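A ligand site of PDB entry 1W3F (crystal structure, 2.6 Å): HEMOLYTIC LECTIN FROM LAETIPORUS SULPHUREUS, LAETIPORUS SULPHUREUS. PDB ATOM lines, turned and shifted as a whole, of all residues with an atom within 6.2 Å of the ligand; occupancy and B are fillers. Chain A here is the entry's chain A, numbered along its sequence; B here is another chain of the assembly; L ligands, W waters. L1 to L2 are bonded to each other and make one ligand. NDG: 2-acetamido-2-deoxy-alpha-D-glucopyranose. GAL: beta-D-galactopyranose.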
ATOM      1  N   ARG A  76       5.704 -24.957  -0.643  1.00  0.00           N
ATOM      2  CA  ARG A  76       6.368 -25.395   0.572  1.00  0.00           C
ATOM      3  C   ARG A  76       7.318 -26.561   0.389  1.00  0.00           C
ATOM      4  O   ARG A  76       8.380 -26.624   1.024  1.00  0.00           O
ATOM      5  CB  ARG A  76       5.350 -25.722   1.672  1.00  0.00           C
ATOM      6  CG  ARG A  76       5.205 -24.587   2.647  1.00  0.00           C
ATOM      7  CD  ARG A  76       6.548 -24.240   3.256  1.00  0.00           C
ATOM      8  NE  ARG A  76       6.594 -22.876   3.753  1.00  0.00           N
ATOM      9  CZ  ARG A  76       7.500 -22.431   4.622  1.00  0.00           C
ATOM     10  NH1 ARG A  76       8.428 -23.250   5.077  1.00  0.00           N
ATOM     11  NH2 ARG A  76       7.477 -21.171   5.022  1.00  0.00           N
ATOM     12  N   GLU A  79      12.514 -26.066  -2.776  1.00  0.00           N
ATOM     13  CA  GLU A  79      13.239 -24.847  -2.460  1.00  0.00           C
ATOM     14  C   GLU A  79      13.764 -24.228  -3.752  1.00  0.00           C
ATOM     15  O   GLU A  79      14.179 -24.943  -4.668  1.00  0.00           O
ATOM     16  CB  GLU A  79      14.405 -25.173  -1.529  1.00  0.00           C
ATOM     17  CG  GLU A  79      14.790 -24.056  -0.579  1.00  0.00           C
ATOM     18  CD  GLU A  79      13.813 -23.906   0.572  1.00  0.00           C
ATOM     19  OE1 GLU A  79      13.738 -24.826   1.427  1.00  0.00           O
ATOM     20  OE2 GLU A  79      13.118 -22.875   0.632  1.00  0.00           O
ATOM     21  N   TYR A  81      11.171 -21.531  -1.718  1.00  0.00           N
ATOM     22  CA  TYR A  81       9.718 -21.458  -1.605  1.00  0.00           C
ATOM     23  C   TYR A  81       9.039 -20.390  -2.466  1.00  0.00           C
ATOM     24  O   TYR A  81       7.849 -20.496  -2.740  1.00  0.00           O
ATOM     25  CB  TYR A  81       9.306 -21.301  -0.145  1.00  0.00           C
ATOM     26  CG  TYR A  81       9.829 -22.395   0.757  1.00  0.00           C
ATOM     27  CD1 TYR A  81      10.170 -23.648   0.255  1.00  0.00           C
ATOM     28  CD2 TYR A  81       9.967 -22.179   2.132  1.00  0.00           C
ATOM     29  CE1 TYR A  81      10.646 -24.657   1.093  1.00  0.00           C
ATOM     30  CE2 TYR A  81      10.435 -23.183   2.969  1.00  0.00           C
ATOM     31  CZ  TYR A  81      10.772 -24.410   2.442  1.00  0.00           C
ATOM     32  OH  TYR A  81      11.253 -25.395   3.276  1.00  0.00           O
ATOM     33  N   LEU A 120       2.533 -15.167   1.290  1.00  0.00           N
ATOM     34  CA  LEU A 120       3.742 -14.405   0.998  1.00  0.00           C
ATOM     35  C   LEU A 120       4.197 -13.584   2.196  1.00  0.00           C
ATOM     36  O   LEU A 120       3.379 -13.068   2.961  1.00  0.00           O
ATOM     37  CB  LEU A 120       3.553 -13.505  -0.223  1.00  0.00           C
ATOM     38  CG  LEU A 120       3.557 -14.244  -1.564  1.00  0.00           C
ATOM     39  CD1 LEU A 120       3.453 -13.252  -2.688  1.00  0.00           C
ATOM     40  CD2 LEU A 120       4.821 -15.084  -1.690  1.00  0.00           C
ATOM     41  N   VAL A 121       5.510 -13.472   2.321  1.00  0.00           N
ATOM     42  CA  VAL A 121       6.142 -12.740   3.411  1.00  0.00           C
ATOM     43  C   VAL A 121       7.050 -11.623   2.895  1.00  0.00           C
ATOM     44  O   VAL A 121       7.793 -11.813   1.910  1.00  0.00           O
ATOM     45  CB  VAL A 121       6.986 -13.712   4.294  1.00  0.00           C
ATOM     46  CG1 VAL A 121       7.773 -12.938   5.337  1.00  0.00           C
ATOM     47  CG2 VAL A 121       6.084 -14.739   4.952  1.00  0.00           C
ATOM     48  N   ARG A 123       9.525  -8.903   4.859  1.00  0.00           N
ATOM     49  CA  ARG A 123      10.107  -8.368   6.097  1.00  0.00           C
ATOM     50  C   ARG A 123      11.579  -7.985   5.939  1.00  0.00           C
ATOM     51  O   ARG A 123      12.241  -8.406   4.991  1.00  0.00           O
ATOM     52  CB  ARG A 123      10.029  -9.447   7.175  1.00  0.00           C
ATOM     53  CG  ARG A 123      10.892 -10.644   6.815  1.00  0.00           C
ATOM     54  CD  ARG A 123      10.508 -11.905   7.547  1.00  0.00           C
ATOM     55  NE  ARG A 123      11.182 -13.044   6.934  1.00  0.00           N
ATOM     56  CZ  ARG A 123      11.050 -14.305   7.324  1.00  0.00           C
ATOM     57  NH1 ARG A 123      10.269 -14.632   8.344  1.00  0.00           N
ATOM     58  NH2 ARG A 123      11.722 -15.259   6.673  1.00  0.00           N
ATOM     59  N   HIS A 125      13.447  -7.774   9.050  1.00  0.00           N
ATOM     60  CA  HIS A 125      13.991  -8.167  10.354  1.00  0.00           C
ATOM     61  C   HIS A 125      14.551  -9.589  10.370  1.00  0.00           C
ATOM     62  O   HIS A 125      15.279  -9.961  11.299  1.00  0.00           O
ATOM     63  CB  HIS A 125      12.897  -8.033  11.430  1.00  0.00           C
ATOM     64  CG  HIS A 125      11.834  -9.084  11.352  1.00  0.00           C
ATOM     65  ND1 HIS A 125      11.809 -10.176  12.195  1.00  0.00           N
ATOM     66  CD2 HIS A 125      10.763  -9.221  10.536  1.00  0.00           C
ATOM     67  CE1 HIS A 125      10.776 -10.945  11.891  1.00  0.00           C
ATOM     68  NE2 HIS A 125      10.125 -10.385  10.881  1.00  0.00           N
ATOM     69  N   LEU A 126      14.226 -10.386   9.360  1.00  0.00           N
ATOM     70  CA  LEU A 126      14.666 -11.775   9.313  1.00  0.00           C
ATOM     71  C   LEU A 126      14.771 -12.242   7.867  1.00  0.00           C
ATOM     72  O   LEU A 126      13.999 -11.822   7.015  1.00  0.00           O
ATOM     73  CB  LEU A 126      13.664 -12.622  10.101  1.00  0.00           C
ATOM     74  CG  LEU A 126      13.795 -14.128  10.342  1.00  0.00           C
ATOM     75  CD1 LEU A 126      13.507 -14.859   9.060  1.00  0.00           C
ATOM     76  CD2 LEU A 126      15.171 -14.466  10.874  1.00  0.00           C
ATOM     77  N   GLN A 127      15.749 -13.100   7.581  1.00  0.00           N
ATOM     78  CA  GLN A 127      15.943 -13.624   6.216  1.00  0.00           C
ATOM     79  C   GLN A 127      15.359 -15.013   6.038  1.00  0.00           C
ATOM     80  O   GLN A 127      15.316 -15.811   6.975  1.00  0.00           O
ATOM     81  CB  GLN A 127      17.429 -13.670   5.864  1.00  0.00           C
ATOM     82  CG  GLN A 127      18.068 -12.322   5.630  1.00  0.00           C
ATOM     83  CD  GLN A 127      19.513 -12.446   5.226  1.00  0.00           C
ATOM     84  OE1 GLN A 127      20.189 -11.449   4.941  1.00  0.00           O
ATOM     85  NE2 GLN A 127      20.023 -13.668   5.188  1.00  0.00           N
ATOM     86  N   PRO A 128      14.897 -15.327   4.813  1.00  0.00           N
ATOM     87  CA  PRO A 128      14.916 -14.425   3.642  1.00  0.00           C
ATOM     88  C   PRO A 128      13.894 -13.309   3.815  1.00  0.00           C
ATOM     89  O   PRO A 128      12.828 -13.501   4.409  1.00  0.00           O
ATOM     90  CB  PRO A 128      14.555 -15.352   2.482  1.00  0.00           C
ATOM     91  CG  PRO A 128      14.945 -16.718   2.972  1.00  0.00           C
ATOM     92  CD  PRO A 128      14.497 -16.682   4.412  1.00  0.00           C
ATOM     93  N   TRP A 131       9.828 -14.140   1.377  1.00  0.00           N
ATOM     94  CA  TRP A 131       9.657 -15.578   1.552  1.00  0.00           C
ATOM     95  C   TRP A 131       8.170 -15.858   1.734  1.00  0.00           C
ATOM     96  O   TRP A 131       7.344 -15.067   1.306  1.00  0.00           O
ATOM     97  CB  TRP A 131      10.411 -15.988   2.828  1.00  0.00           C
ATOM     98  CG  TRP A 131      10.947 -17.376   2.837  1.00  0.00           C
ATOM     99  CD1 TRP A 131      10.818 -18.290   3.850  1.00  0.00           C
ATOM    100  CD2 TRP A 131      11.756 -17.993   1.841  1.00  0.00           C
ATOM    101  NE1 TRP A 131      11.493 -19.440   3.531  1.00  0.00           N
ATOM    102  CE2 TRP A 131      12.089 -19.284   2.304  1.00  0.00           C
ATOM    103  CE3 TRP A 131      12.240 -17.582   0.590  1.00  0.00           C
ATOM    104  CZ2 TRP A 131      12.872 -20.175   1.570  1.00  0.00           C
ATOM    105  CZ3 TRP A 131      13.031 -18.463  -0.151  1.00  0.00           C
ATOM    106  CH2 TRP A 131      13.339 -19.736   0.343  1.00  0.00           C
ATOM    107  N   ASN A 132       7.838 -17.004   2.329  1.00  0.00           N
ATOM    108  CA  ASN A 132       6.441 -17.307   2.600  1.00  0.00           C
ATOM    109  C   ASN A 132       6.312 -18.004   3.947  1.00  0.00           C
ATOM    110  O   ASN A 132       7.309 -18.296   4.590  1.00  0.00           O
ATOM    111  CB  ASN A 132       5.762 -18.141   1.494  1.00  0.00           C
ATOM    112  CG  ASN A 132       6.273 -19.572   1.401  1.00  0.00           C
ATOM    113  OD1 ASN A 132       6.684 -20.178   2.393  1.00  0.00           O
ATOM    114  ND2 ASN A 132       6.206 -20.125   0.187  1.00  0.00           N
ATOM    115  N   HIS A 133       5.083 -18.247   4.381  1.00  0.00           N
ATOM    116  CA  HIS A 133       4.826 -18.836   5.683  1.00  0.00           C
ATOM    117  C   HIS A 133       3.530 -19.661   5.629  1.00  0.00           C
ATOM    118  O   HIS A 133       2.684 -19.451   4.757  1.00  0.00           O
ATOM    119  CB  HIS A 133       4.691 -17.702   6.703  1.00  0.00           C
ATOM    120  CG  HIS A 133       4.807 -18.135   8.125  1.00  0.00           C
ATOM    121  ND1 HIS A 133       5.990 -18.588   8.665  1.00  0.00           N
ATOM    122  CD2 HIS A 133       3.892 -18.169   9.126  1.00  0.00           C
ATOM    123  CE1 HIS A 133       5.802 -18.891   9.941  1.00  0.00           C
ATOM    124  NE2 HIS A 133       4.538 -18.641  10.242  1.00  0.00           N
ATOM    125  N   GLU A 137      -0.752 -19.382  10.207  1.00  0.00           N
ATOM    126  CA  GLU A 137      -0.150 -18.510  11.199  1.00  0.00           C
ATOM    127  C   GLU A 137      -0.005 -17.109  10.583  1.00  0.00           C
ATOM    128  O   GLU A 137       0.881 -16.877   9.765  1.00  0.00           O
ATOM    129  CB  GLU A 137       1.233 -19.020  11.613  1.00  0.00           C
ATOM    130  CG  GLU A 137       1.320 -19.492  13.050  1.00  0.00           C
ATOM    131  CD  GLU A 137       2.681 -19.223  13.664  1.00  0.00           C
ATOM    132  OE1 GLU A 137       3.695 -19.606  13.055  1.00  0.00           O
ATOM    133  OE2 GLU A 137       2.743 -18.618  14.762  1.00  0.00           O
ATOM    134  N   VAL A 138      -0.862 -16.193  10.988  1.00  0.00           N
ATOM    135  CA  VAL A 138      -0.844 -14.844  10.455  1.00  0.00           C
ATOM    136  C   VAL A 138       0.015 -13.834  11.226  1.00  0.00           C
ATOM    137  O   VAL A 138      -0.183 -13.621  12.424  1.00  0.00           O
ATOM    138  CB  VAL A 138      -2.285 -14.269  10.373  1.00  0.00           C
ATOM    139  CG1 VAL A 138      -2.287 -12.966   9.621  1.00  0.00           C
ATOM    140  CG2 VAL A 138      -3.207 -15.274   9.693  1.00  0.00           C
ATOM    141  N   PHE A 139       0.963 -13.230  10.521  1.00  0.00           N
ATOM    142  CA  PHE A 139       1.848 -12.200  11.082  1.00  0.00           C
ATOM    143  C   PHE A 139       1.709 -10.960  10.216  1.00  0.00           C
ATOM    144  O   PHE A 139       1.405 -11.050   9.025  1.00  0.00           O
ATOM    145  CB  PHE A 139       3.311 -12.648  11.075  1.00  0.00           C
ATOM    146  CG  PHE A 139       3.662 -13.643  12.141  1.00  0.00           C
ATOM    147  CD1 PHE A 139       3.641 -15.007  11.873  1.00  0.00           C
ATOM    148  CD2 PHE A 139       4.061 -13.208  13.393  1.00  0.00           C
ATOM    149  CE1 PHE A 139       4.027 -15.924  12.851  1.00  0.00           C
ATOM    150  CE2 PHE A 139       4.442 -14.114  14.384  1.00  0.00           C
ATOM    151  CZ  PHE A 139       4.421 -15.477  14.116  1.00  0.00           C
ATOM    152  N   ASP A 140       1.945  -9.788  10.795  1.00  0.00           N
ATOM    153  CA  ASP A 140       1.835  -8.533  10.057  1.00  0.00           C
ATOM    154  C   ASP A 140       2.708  -8.421   8.822  1.00  0.00           C
ATOM    155  O   ASP A 140       2.366  -7.696   7.889  1.00  0.00           O
ATOM    156  CB  ASP A 140       2.142  -7.337  10.977  1.00  0.00           C
ATOM    157  CG  ASP A 140       0.950  -6.894  11.792  1.00  0.00           C
ATOM    158  OD1 ASP A 140      -0.185  -7.323  11.489  1.00  0.00           O
ATOM    159  OD2 ASP A 140       1.136  -6.091  12.739  1.00  0.00           O
ATOM    160  N   ASP A 141       3.837  -9.132   8.792  1.00  0.00           N
ATOM    161  CA  ASP A 141       4.724  -9.045   7.650  1.00  0.00           C
ATOM    162  C   ASP A 141       4.243  -9.800   6.432  1.00  0.00           C
ATOM    163  O   ASP A 141       4.978  -9.965   5.462  1.00  0.00           O
ATOM    164  CB  ASP A 141       6.158  -9.489   8.009  1.00  0.00           C
ATOM    165  CG  ASP A 141       6.222 -10.868   8.660  1.00  0.00           C
ATOM    166  OD1 ASP A 141       5.283 -11.683   8.493  1.00  0.00           O
ATOM    167  OD2 ASP A 141       7.235 -11.134   9.335  1.00  0.00           O
ATOM    168  N   GLN A 142       3.004 -10.260   6.488  1.00  0.00           N
ATOM    169  CA  GLN A 142       2.388 -10.988   5.393  1.00  0.00           C
ATOM    170  C   GLN A 142       1.466 -10.048   4.619  1.00  0.00           C
ATOM    171  O   GLN A 142       0.838 -10.440   3.631  1.00  0.00           O
ATOM    172  CB  GLN A 142       1.570 -12.165   5.936  1.00  0.00           C
ATOM    173  CG  GLN A 142       2.388 -13.430   6.194  1.00  0.00           C
ATOM    174  CD  GLN A 142       1.730 -14.364   7.202  1.00  0.00           C
ATOM    175  OE1 GLN A 142       0.524 -14.577   7.171  1.00  0.00           O
ATOM    176  NE2 GLN A 142       2.521 -14.926   8.085  1.00  0.00           N
ATOM    177  N   SER B  37       8.468  -9.315  18.345  1.00  0.00           N
ATOM    178  CA  SER B  37       7.874 -10.062  17.260  1.00  0.00           C
ATOM    179  C   SER B  37       6.806  -9.310  16.498  1.00  0.00           C
ATOM    180  O   SER B  37       6.108  -8.451  17.053  1.00  0.00           O
ATOM    181  CB  SER B  37       7.234 -11.354  17.785  1.00  0.00           C
ATOM    182  OG  SER B  37       6.370 -11.904  16.793  1.00  0.00           O
ATOM    183  N   PRO B  38       6.680  -9.605  15.200  1.00  0.00           N
ATOM    184  CA  PRO B  38       5.673  -8.945  14.375  1.00  0.00           C
ATOM    185  C   PRO B  38       4.350  -9.409  14.994  1.00  0.00           C
ATOM    186  O   PRO B  38       4.301 -10.486  15.601  1.00  0.00           O
ATOM    187  CB  PRO B  38       5.892  -9.557  12.993  1.00  0.00           C
ATOM    188  CG  PRO B  38       7.356  -9.882  12.997  1.00  0.00           C
ATOM    189  CD  PRO B  38       7.564 -10.449  14.374  1.00  0.00           C
HETATM  190  C1  NDG L   1      11.839 -20.815   9.531  1.00  0.00           C
HETATM  191  C2  NDG L   1      11.499 -19.719   8.451  1.00  0.00           C
HETATM  192  C3  NDG L   1      11.247 -18.406   9.214  1.00  0.00           C
HETATM  193  C4  NDG L   1      10.085 -18.563  10.207  1.00  0.00           C
HETATM  194  C5  NDG L   1      10.365 -19.766  11.212  1.00  0.00           C
HETATM  195  C6  NDG L   1       9.169 -20.354  11.946  1.00  0.00           C
HETATM  196  C7  NDG L   1      12.727 -20.345   6.418  1.00  0.00           C
HETATM  197  C8  NDG L   1      13.950 -20.056   5.559  1.00  0.00           C
HETATM  198  O5  NDG L   1      10.744 -20.901  10.432  1.00  0.00           O
HETATM  199  O3  NDG L   1      10.934 -17.345   8.323  1.00  0.00           O
HETATM  200  O4  NDG L   1       9.955 -17.311  10.887  1.00  0.00           O
HETATM  201  O6  NDG L   1       8.630 -19.478  12.746  1.00  0.00           O
HETATM  202  O7  NDG L   1      11.900 -21.255   6.116  1.00  0.00           O
HETATM  203  N2  NDG L   1      12.607 -19.564   7.518  1.00  0.00           N
HETATM  204  O1  NDG L   1      12.996 -20.513  10.242  1.00  0.00           O
HETATM  205  C1  GAL L   2       8.856 -16.521  10.924  1.00  0.00           C
HETATM  206  C2  GAL L   2       9.140 -15.382  11.983  1.00  0.00           C
HETATM  207  C3  GAL L   2       7.969 -14.357  12.128  1.00  0.00           C
HETATM  208  C4  GAL L   2       7.377 -13.967  10.759  1.00  0.00           C
HETATM  209  C5  GAL L   2       7.027 -15.234   9.926  1.00  0.00           C
HETATM  210  C6  GAL L   2       6.422 -14.878   8.567  1.00  0.00           C
HETATM  211  O2  GAL L   2       9.411 -15.900  13.293  1.00  0.00           O
HETATM  212  O3  GAL L   2       8.447 -13.184  12.797  1.00  0.00           O
HETATM  213  O4  GAL L   2       8.328 -13.186  10.059  1.00  0.00           O
HETATM  214  O5  GAL L   2       8.192 -16.045   9.741  1.00  0.00           O
HETATM  215  O6  GAL L   2       5.090 -14.479   8.688  1.00  0.00           O
HETATM  216  O   HOH W   1      12.060 -16.493  14.184  1.00  0.00           O
HETATM  217  O   HOH W   2       8.127 -13.907  15.471  1.00  0.00           O
HETATM  218  O   HOH W   3       8.171 -18.570   7.234  1.00  0.00           O
HETATM  219  O   HOH W   4      14.895 -17.933   8.631  1.00  0.00           O
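NE2 of Gln 142 is in hydrogen-bond range of O of Glu 137. The backbone NH of Phe 139 sits close to the side-chain amide nitrogen of Gln 142 (3.4 Å). The guanidinium group (NE) of Arg 123 sits at hydrogen-bond distance from the backbone carbonyl oxygen (O) of Pro 128 (3.0 Å). A ring nitrogen (NE2) of His 125 lies within hydrogen-bond range of the side-chain carboxylate (OD2) of Asp 141 (3.4 Å). NE of Arg 123 is in hydrogen-bond range of O of Leu 126 (3.1 Å). N of Val 121 lies within hydrogen-bond range of O of Trp 131. The side-chain amide nitrogen of Asn 132 lies close to the backbone carbonyl oxygen of Tyr 81 (3.4 Å). A ring nitrogen (NE2) of His 133 is in hydrogen-bond range of the side-chain carboxylate (OE1) of Glu 137 (3.1 Å).
NH2 of Arg 123 lies within hydrogen-bond range of O3 of NDG L1. O6 of GAL L2 lies within hydrogen-bond range of NE2 of Gln 142, at 2.7 Å. An oxygen (O7) of NDG L1 lies within hydrogen-bond range of the indole nitrogen of Trp 131. OD2 of Asp 141 is in hydrogen-bond range of O4 of GAL L2 (2.4 Å). NE2 of His 125 sits at hydrogen-bond distance from O4 of GAL L2, at 3.4 Å.
Water W2 bridges an oxygen (O3) of GAL L2 (2.8 Å) and the side-chain hydroxyl of Ser 37 of chain B (3.0 Å). Water W4 bridges O of Gln 127 (2.7 Å) and N2 of NDG L1 (3.0 Å). Water W3 lies within hydrogen-bond range of a ring nitrogen (ND1) of His 133, the backbone carbonyl oxygen of Asn 132, an oxygen (O3) of NDG L1 and the guanidinium group of Arg 76.
CE2 of Tyr 81 touches O7 of NDG L1, at 3.97 Å. CG2 of Val 121 touches C6 of GAL L2 (3.6 Å). CD1 of Leu 126 touches O3 of NDG L1, 3.7 Å away. Pro 128 touches the ligand. ND1 of His 133 touches O5 of GAL L2, 3.5 Å away. CB of Phe 139 touches O6 of GAL L2, 3.5 Å away. Pro 38 of chain B touches the ligand. Hydrophobic or aromatic side chains that line the ligand: Tyr 81, Val 121, His 125, Leu 126, Pro 128, Trp 131, His 133, Phe 139 and Pro 38 of chain B. 12 residues have an atom within 4 Å of the ligand: Tyr 81, Val 121, Arg 123, His 125, Leu 126, Pro 128, Trp 131, His 133, Phe 139, Asp 141, Gln 142 and Pro 38 of chain B. The nearest printed residue that does not touch the ligand is Arg 76 (4.1 Å).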
